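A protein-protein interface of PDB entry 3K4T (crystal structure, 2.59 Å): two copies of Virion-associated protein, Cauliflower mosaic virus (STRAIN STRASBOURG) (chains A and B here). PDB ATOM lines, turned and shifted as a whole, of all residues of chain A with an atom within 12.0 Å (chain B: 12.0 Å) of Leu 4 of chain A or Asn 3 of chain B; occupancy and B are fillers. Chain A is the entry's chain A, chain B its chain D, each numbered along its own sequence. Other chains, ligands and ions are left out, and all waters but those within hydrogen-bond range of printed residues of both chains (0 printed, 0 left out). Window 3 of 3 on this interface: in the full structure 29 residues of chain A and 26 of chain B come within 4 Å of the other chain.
OE1 of Gln 8 of chain A sits close to OE1 of Gln 6 of chain B (2.6 Å). The side-chain amide nitrogen of Gln 8 of chain A sits at hydrogen-bond distance from the side-chain carboxylate of Glu 10 of chain B (3.1 Å). The side-chain carboxylate of Glu 10 of chain B sits at hydrogen-bond distance from the side-chain hydroxyl of Ser 12 of chain A (3.0 Å).
The side-chain amide nitrogen of Gln 8 of chain A lies within hydrogen-bond range of the side-chain hydroxyl of Ser 12 of chain A, at 3.3 Å. The side-chain amide oxygen (OD1) of Asn 3 of chain B sits close to the side-chain amide oxygen (OE1) of Gln 6 of chain B (3.5 Å).
Among the printed residues, merely in contact across the chains: Leu 4 of chain A with Asn 3 of chain B (3.4 Å), Leu 4 of chain A with Ile 7 of chain B (3.7 Å), Ile 7 of chain A with Ile 7 of chain B (3.997 Å), Gln 8 of chain A with Ile 7 of chain B (3.1 Å), Val 11 of chain A with Glu 10 of chain B (3.3 Å), Val 11 of chain A with Ile 14 of chain B (3.7 Å) and Ile 14 of chain A with Ile 14 of chain B (3.9 Å).
Leu 4 of chain A touches just these residues of chain B: Asn 3 and Ile 7. Printed residues of chain A within 4 Å of Asn 3 of chain B: Leu 4. No residue of chain B comes within 4 Å of Ala 2 of chain A. No residue of chain B comes within 4 Å of Asn 3 of chain A. No residue of chain A comes within 4 Å of Leu 4 of chain B. Printed residues of chain A within 4 Å of Gln 6 of chain B: Gln 8. Of the printed residues of chain A, Glu 10 of chain B touches Gln 8, Val 11 and Ser 12. Printed residues of chain B within 4 Å of Val 11 of chain A: Glu 10 (3.3 Å) and Ile 14 (3.7 Å). Of the printed residues of chain A, Ile 14 of chain B touches Val 11 (3.7 Å) and Ile 14 (3.9 Å). Of the printed residues of chain A, Ile 7 of chain B touches Leu 4, Ile 7 and Gln 8. Printed residues of chain B within 4 Å of Ile 7 of chain A: Ile 7 (3.997 Å). Ser 12 of chain B touches none of the printed residues of chain A. Glu 10 of chain A touches none of the printed residues of chain B. The nearest printed residue of chain A that does not touch Asn 3 of chain B is Gln 8 of chain A (4.01 Å).
Printed residues of chain A that touch a printed residue of chain B: Leu 4, Ile 7, Gln 8, Val 11, Ser 12 and Ile 14. Hydrophobic or aromatic side chains of chain B that line the printed part of chain A: Ile 7 and Ile 14. Along chain B the printed residues that touch a printed residue of chain A span positions 3 to 14. Among the printed residues, 10 pairs touch across the chains.
Ile 7 of chain B touches its own counterpart, Ile 7 of chain A. Gln 8 of chain A touches Gln 6 of chain B, but with the chains exchanged Gln 6 of chain A does not touch Gln 8 of chain B (11.9 Å). Val 11 of chain A touches Glu 10 of chain B, but with the chains exchanged Glu 10 of chain A does not touch Val 11 of chain B (8.4 Å). Ile 14 of chain B touches its own counterpart, Ile 14 of chain A. Of the 10 pairs that touch across the chains among the printed residues, 2 have their exchanged pair printed and touching as well.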
ATOM      1  N   ALA A   2     -11.651 -27.610  15.922  1.00  0.00           N
ATOM      2  CA  ALA A   2     -10.421 -26.954  15.353  1.00  0.00           C
ATOM      3  C   ALA A   2     -10.262 -27.270  13.855  1.00  0.00           C
ATOM      4  O   ALA A   2      -9.740 -26.461  13.079  1.00  0.00           O
ATOM      5  CB  ALA A   2      -9.172 -27.374  16.157  1.00  0.00           C
ATOM      6  N   ASN A   3     -10.748 -28.457  13.482  1.00  0.00           N
ATOM      7  CA  ASN A   3     -10.819 -28.949  12.109  1.00  0.00           C
ATOM      8  C   ASN A   3     -11.613 -28.045  11.172  1.00  0.00           C
ATOM      9  O   ASN A   3     -11.109 -27.640  10.125  1.00  0.00           O
ATOM     10  CB  ASN A   3     -11.447 -30.354  12.100  1.00  0.00           C
ATOM     11  CG  ASN A   3     -10.432 -31.454  11.919  1.00  0.00           C
ATOM     12  OD1 ASN A   3      -9.232 -31.248  12.110  1.00  0.00           O
ATOM     13  ND2 ASN A   3     -10.898 -32.631  11.542  1.00  0.00           N
ATOM     14  N   LEU A   4     -12.847 -27.727  11.556  1.00  0.00           N
ATOM     15  CA  LEU A   4     -13.764 -26.994  10.693  1.00  0.00           C
ATOM     16  C   LEU A   4     -13.310 -25.570  10.432  1.00  0.00           C
ATOM     17  O   LEU A   4     -13.522 -25.039   9.331  1.00  0.00           O
ATOM     18  CB  LEU A   4     -15.172 -26.987  11.280  1.00  0.00           C
ATOM     19  CG  LEU A   4     -16.302 -26.928  10.254  1.00  0.00           C
ATOM     20  CD1 LEU A   4     -16.106 -27.974   9.158  1.00  0.00           C
ATOM     21  CD2 LEU A   4     -17.652 -27.117  10.924  1.00  0.00           C
ATOM     22  N   ASN A   5     -12.698 -24.959  11.451  1.00  0.00           N
ATOM     23  CA  ASN A   5     -12.160 -23.609  11.334  1.00  0.00           C
ATOM     24  C   ASN A   5     -11.006 -23.503  10.354  1.00  0.00           C
ATOM     25  O   ASN A   5     -10.988 -22.606   9.521  1.00  0.00           O
ATOM     26  CB  ASN A   5     -11.746 -23.060  12.696  1.00  0.00           C
ATOM     27  CG  ASN A   5     -12.867 -22.325  13.382  1.00  0.00           C
ATOM     28  OD1 ASN A   5     -13.937 -22.890  13.622  1.00  0.00           O
ATOM     29  ND2 ASN A   5     -12.635 -21.050  13.703  1.00  0.00           N
ATOM     30  N   GLN A   6     -10.046 -24.416  10.449  1.00  0.00           N
ATOM     31  CA  GLN A   6      -8.986 -24.475   9.457  1.00  0.00           C
ATOM     32  C   GLN A   6      -9.579 -24.558   8.046  1.00  0.00           C
ATOM     33  O   GLN A   6      -9.186 -23.797   7.162  1.00  0.00           O
ATOM     34  CB  GLN A   6      -8.014 -25.626   9.735  1.00  0.00           C
ATOM     35  CG  GLN A   6      -6.775 -25.609   8.840  1.00  0.00           C
ATOM     36  CD  GLN A   6      -5.486 -25.786   9.607  1.00  0.00           C
ATOM     37  OE1 GLN A   6      -5.441 -26.469  10.637  1.00  0.00           O
ATOM     38  NE2 GLN A   6      -4.418 -25.162   9.113  1.00  0.00           N
ATOM     39  N   ILE A   7     -10.544 -25.447   7.838  1.00  0.00           N
ATOM     40  CA  ILE A   7     -11.201 -25.523   6.527  1.00  0.00           C
ATOM     41  C   ILE A   7     -11.886 -24.201   6.189  1.00  0.00           C
ATOM     42  O   ILE A   7     -11.698 -23.665   5.100  1.00  0.00           O
ATOM     43  CB  ILE A   7     -12.188 -26.705   6.403  1.00  0.00           C
ATOM     44  CG1 ILE A   7     -11.485 -28.020   6.737  1.00  0.00           C
ATOM     45  CG2 ILE A   7     -12.787 -26.740   4.999  1.00  0.00           C
ATOM     46  CD1 ILE A   7     -12.433 -29.160   6.955  1.00  0.00           C
ATOM     47  N   GLN A   8     -12.650 -23.660   7.129  1.00  0.00           N
ATOM     48  CA  GLN A   8     -13.249 -22.342   6.944  1.00  0.00           C
ATOM     49  C   GLN A   8     -12.235 -21.249   6.540  1.00  0.00           C
ATOM     50  O   GLN A   8     -12.515 -20.475   5.624  1.00  0.00           O
ATOM     51  CB  GLN A   8     -14.046 -21.932   8.186  1.00  0.00           C
ATOM     52  CG  GLN A   8     -14.737 -20.575   8.066  1.00  0.00           C
ATOM     53  CD  GLN A   8     -15.502 -20.425   6.767  1.00  0.00           C
ATOM     54  OE1 GLN A   8     -16.461 -21.153   6.509  1.00  0.00           O
ATOM     55  NE2 GLN A   8     -15.083 -19.478   5.940  1.00  0.00           N
ATOM     56  N   LYS A   9     -11.074 -21.197   7.207  1.00  0.00           N
ATOM     57  CA  LYS A   9      -9.999 -20.223   6.895  1.00  0.00           C
ATOM     58  C   LYS A   9      -9.499 -20.329   5.457  1.00  0.00           C
ATOM     59  O   LYS A   9      -9.425 -19.333   4.742  1.00  0.00           O
ATOM     60  CB  LYS A   9      -8.778 -20.421   7.803  1.00  0.00           C
ATOM     61  CG  LYS A   9      -8.803 -19.767   9.168  1.00  0.00           C
ATOM     62  CD  LYS A   9      -7.492 -20.092   9.885  1.00  0.00           C
ATOM     63  CE  LYS A   9      -7.721 -20.454  11.345  1.00  0.00           C
ATOM     64  NZ  LYS A   9      -7.790 -19.234  12.205  1.00  0.00           N
ATOM     65  N   GLU A  10      -9.138 -21.545   5.057  1.00  0.00           N
ATOM     66  CA  GLU A  10      -8.557 -21.795   3.753  1.00  0.00           C
ATOM     67  C   GLU A  10      -9.558 -21.572   2.663  1.00  0.00           C
ATOM     68  O   GLU A  10      -9.196 -21.126   1.585  1.00  0.00           O
ATOM     69  CB  GLU A  10      -8.016 -23.212   3.657  1.00  0.00           C
ATOM     70  CG  GLU A  10      -6.973 -23.537   4.720  1.00  0.00           C
ATOM     71  CD  GLU A  10      -6.002 -24.617   4.285  1.00  0.00           C
ATOM     72  OE1 GLU A  10      -6.417 -25.587   3.613  1.00  0.00           O
ATOM     73  OE2 GLU A  10      -4.803 -24.488   4.624  1.00  0.00           O
ATOM     74  N   VAL A  11     -10.819 -21.880   2.941  1.00  0.00           N
ATOM     75  CA  VAL A  11     -11.881 -21.701   1.956  1.00  0.00           C
ATOM     76  C   VAL A  11     -12.110 -20.216   1.676  1.00  0.00           C
ATOM     77  O   VAL A  11     -12.237 -19.815   0.514  1.00  0.00           O
ATOM     78  CB  VAL A  11     -13.190 -22.435   2.373  1.00  0.00           C
ATOM     79  CG1 VAL A  11     -14.397 -21.815   1.712  1.00  0.00           C
ATOM     80  CG2 VAL A  11     -13.092 -23.947   2.044  1.00  0.00           C
ATOM     81  N   SER A  12     -12.145 -19.417   2.745  1.00  0.00           N
ATOM     82  CA  SER A  12     -12.251 -17.961   2.654  1.00  0.00           C
ATOM     83  C   SER A  12     -11.105 -17.373   1.853  1.00  0.00           C
ATOM     84  O   SER A  12     -11.308 -16.470   1.051  1.00  0.00           O
ATOM     85  CB  SER A  12     -12.258 -17.334   4.051  1.00  0.00           C
ATOM     86  OG  SER A  12     -13.561 -16.928   4.427  1.00  0.00           O
ATOM     87  N   GLU A  13      -9.906 -17.902   2.085  1.00  0.00           N
ATOM     88  CA  GLU A  13      -8.690 -17.448   1.416  1.00  0.00           C
ATOM     89  C   GLU A  13      -8.697 -17.792  -0.067  1.00  0.00           C
ATOM     90  O   GLU A  13      -8.319 -16.944  -0.873  1.00  0.00           O
ATOM     91  CB  GLU A  13      -7.432 -18.000   2.102  1.00  0.00           C
ATOM     92  CG  GLU A  13      -6.118 -17.584   1.439  1.00  0.00           C
ATOM     93  CD  GLU A  13      -4.889 -18.131   2.151  1.00  0.00           C
ATOM     94  OE1 GLU A  13      -5.035 -19.118   2.910  1.00  0.00           O
ATOM     95  OE2 GLU A  13      -3.776 -17.584   1.951  1.00  0.00           O
ATOM     96  N   ILE A  14      -9.121 -19.011  -0.425  1.00  0.00           N
ATOM     97  CA  ILE A  14      -9.273 -19.392  -1.830  1.00  0.00           C
ATOM     98  C   ILE A  14     -10.175 -18.395  -2.537  1.00  0.00           C
ATOM     99  O   ILE A  14      -9.786 -17.844  -3.563  1.00  0.00           O
ATOM    100  CB  ILE A  14      -9.831 -20.859  -2.057  1.00  0.00           C
ATOM    101  CG1 ILE A  14      -8.838 -21.927  -1.591  1.00  0.00           C
ATOM    102  CG2 ILE A  14     -10.076 -21.125  -3.529  1.00  0.00           C
ATOM    103  CD1 ILE A  14      -9.456 -23.265  -1.244  1.00  0.00           C
ATOM    104  N   ASN B   3     -21.221 -22.946  10.686  1.00  0.00           N
ATOM    105  CA  ASN B   3     -19.920 -23.312  10.037  1.00  0.00           C
ATOM    106  C   ASN B   3     -20.042 -24.171   8.763  1.00  0.00           C
ATOM    107  O   ASN B   3     -19.472 -23.800   7.745  1.00  0.00           O
ATOM    108  CB  ASN B   3     -18.951 -23.937  11.048  1.00  0.00           C
ATOM    109  CG  ASN B   3     -17.900 -22.948  11.561  1.00  0.00           C
ATOM    110  OD1 ASN B   3     -17.035 -22.480  10.809  1.00  0.00           O
ATOM    111  ND2 ASN B   3     -17.950 -22.658  12.857  1.00  0.00           N
ATOM    112  N   LEU B   4     -20.780 -25.283   8.779  1.00  0.00           N
ATOM    113  CA  LEU B   4     -20.836 -26.141   7.575  1.00  0.00           C
ATOM    114  C   LEU B   4     -21.593 -25.509   6.395  1.00  0.00           C
ATOM    115  O   LEU B   4     -21.056 -25.419   5.296  1.00  0.00           O
ATOM    116  CB  LEU B   4     -21.370 -27.548   7.885  1.00  0.00           C
ATOM    117  CG  LEU B   4     -21.063 -28.704   6.911  1.00  0.00           C
ATOM    118  CD1 LEU B   4     -19.583 -29.037   6.838  1.00  0.00           C
ATOM    119  CD2 LEU B   4     -21.822 -29.980   7.261  1.00  0.00           C
ATOM    120  N   ASN B   5     -22.831 -25.066   6.607  1.00  0.00           N
ATOM    121  CA  ASN B   5     -23.565 -24.399   5.527  1.00  0.00           C
ATOM    122  C   ASN B   5     -22.877 -23.158   4.990  1.00  0.00           C
ATOM    123  O   ASN B   5     -22.928 -22.903   3.793  1.00  0.00           O
ATOM    124  CB  ASN B   5     -25.006 -24.086   5.906  1.00  0.00           C
ATOM    125  CG  ASN B   5     -25.999 -25.056   5.274  1.00  0.00           C
ATOM    126  OD1 ASN B   5     -26.111 -26.210   5.705  1.00  0.00           O
ATOM    127  ND2 ASN B   5     -26.732 -24.590   4.253  1.00  0.00           N
ATOM    128  N   GLN B   6     -22.240 -22.397   5.881  1.00  0.00           N
ATOM    129  CA  GLN B   6     -21.277 -21.359   5.495  1.00  0.00           C
ATOM    130  C   GLN B   6     -20.238 -21.869   4.485  1.00  0.00           C
ATOM    131  O   GLN B   6     -20.023 -21.241   3.435  1.00  0.00           O
ATOM    132  CB  GLN B   6     -20.564 -20.837   6.743  1.00  0.00           C
ATOM    133  CG  GLN B   6     -19.571 -19.688   6.518  1.00  0.00           C
ATOM    134  CD  GLN B   6     -18.753 -19.369   7.778  1.00  0.00           C
ATOM    135  OE1 GLN B   6     -18.071 -20.251   8.323  1.00  0.00           O
ATOM    136  NE2 GLN B   6     -18.819 -18.109   8.242  1.00  0.00           N
ATOM    137  N   ILE B   7     -19.595 -23.004   4.801  1.00  0.00           N
ATOM    138  CA  ILE B   7     -18.544 -23.562   3.946  1.00  0.00           C
ATOM    139  C   ILE B   7     -19.095 -24.016   2.589  1.00  0.00           C
ATOM    140  O   ILE B   7     -18.539 -23.672   1.544  1.00  0.00           O
ATOM    141  CB  ILE B   7     -17.740 -24.693   4.656  1.00  0.00           C
ATOM    142  CG1 ILE B   7     -16.907 -24.111   5.815  1.00  0.00           C
ATOM    143  CG2 ILE B   7     -16.843 -25.432   3.668  1.00  0.00           C
ATOM    144  CD1 ILE B   7     -16.071 -25.127   6.609  1.00  0.00           C
ATOM    145  N   GLN B   8     -20.198 -24.761   2.615  1.00  0.00           N
ATOM    146  CA  GLN B   8     -20.872 -25.221   1.407  1.00  0.00           C
ATOM    147  C   GLN B   8     -21.218 -24.082   0.450  1.00  0.00           C
ATOM    148  O   GLN B   8     -21.195 -24.246  -0.769  1.00  0.00           O
ATOM    149  CB  GLN B   8     -22.117 -26.018   1.785  1.00  0.00           C
ATOM    150  CG  GLN B   8     -23.247 -25.993   0.767  1.00  0.00           C
ATOM    151  CD  GLN B   8     -22.826 -26.449  -0.616  1.00  0.00           C
ATOM    152  OE1 GLN B   8     -23.409 -26.032  -1.616  1.00  0.00           O
ATOM    153  NE2 GLN B   8     -21.810 -27.292  -0.683  1.00  0.00           N
ATOM    154  N   LYS B   9     -21.517 -22.919   1.002  1.00  0.00           N
ATOM    155  CA  LYS B   9     -21.793 -21.750   0.186  1.00  0.00           C
ATOM    156  C   LYS B   9     -20.485 -21.177  -0.432  1.00  0.00           C
ATOM    157  O   LYS B   9     -20.401 -20.981  -1.653  1.00  0.00           O
ATOM    158  CB  LYS B   9     -22.628 -20.731   0.987  1.00  0.00           C
ATOM    159  CG  LYS B   9     -22.642 -19.314   0.456  1.00  0.00           C
ATOM    160  CD  LYS B   9     -23.248 -18.382   1.501  1.00  0.00           C
ATOM    161  CE  LYS B   9     -23.044 -16.909   1.132  1.00  0.00           C
ATOM    162  NZ  LYS B   9     -23.895 -16.011   1.985  1.00  0.00           N
ATOM    163  N   GLU B  10     -19.455 -20.942   0.376  1.00  0.00           N
ATOM    164  CA  GLU B  10     -18.177 -20.506  -0.215  1.00  0.00           C
ATOM    165  C   GLU B  10     -17.624 -21.485  -1.226  1.00  0.00           C
ATOM    166  O   GLU B  10     -16.944 -21.074  -2.160  1.00  0.00           O
ATOM    167  CB  GLU B  10     -17.109 -20.231   0.825  1.00  0.00           C
ATOM    168  CG  GLU B  10     -17.191 -18.872   1.431  1.00  0.00           C
ATOM    169  CD  GLU B  10     -16.793 -18.909   2.880  1.00  0.00           C
ATOM    170  OE1 GLU B  10     -17.052 -19.940   3.543  1.00  0.00           O
ATOM    171  OE2 GLU B  10     -16.230 -17.916   3.369  1.00  0.00           O
ATOM    172  N   VAL B  11     -17.908 -22.767  -1.043  1.00  0.00           N
ATOM    173  CA  VAL B  11     -17.449 -23.783  -1.984  1.00  0.00           C
ATOM    174  C   VAL B  11     -18.204 -23.643  -3.317  1.00  0.00           C
ATOM    175  O   VAL B  11     -17.584 -23.644  -4.384  1.00  0.00           O
ATOM    176  CB  VAL B  11     -17.506 -25.242  -1.370  1.00  0.00           C
ATOM    177  CG1 VAL B  11     -17.336 -26.300  -2.422  1.00  0.00           C
ATOM    178  CG2 VAL B  11     -16.410 -25.415  -0.347  1.00  0.00           C
ATOM    179  N   SER B  12     -19.533 -23.498  -3.258  1.00  0.00           N
ATOM    180  CA  SER B  12     -20.319 -23.271  -4.472  1.00  0.00           C
ATOM    181  C   SER B  12     -19.828 -22.026  -5.168  1.00  0.00           C
ATOM    182  O   SER B  12     -19.749 -21.989  -6.390  1.00  0.00           O
ATOM    183  CB  SER B  12     -21.803 -23.143  -4.169  1.00  0.00           C
ATOM    184  OG  SER B  12     -22.321 -24.377  -3.720  1.00  0.00           O
ATOM    185  N   ILE B  14     -16.706 -20.576  -4.910  1.00  0.00           N
ATOM    186  CA  ILE B  14     -15.414 -20.910  -5.551  1.00  0.00           C
ATOM    187  C   ILE B  14     -15.612 -21.642  -6.879  1.00  0.00           C
ATOM    188  O   ILE B  14     -14.959 -21.320  -7.861  1.00  0.00           O
ATOM    189  CB  ILE B  14     -14.463 -21.756  -4.644  1.00  0.00           C
ATOM    190  CG1 ILE B  14     -14.002 -20.945  -3.445  1.00  0.00           C
ATOM    191  CG2 ILE B  14     -13.248 -22.227  -5.428  1.00  0.00           C
ATOM    192  CD1 ILE B  14     -13.760 -21.784  -2.251  1.00  0.00           C
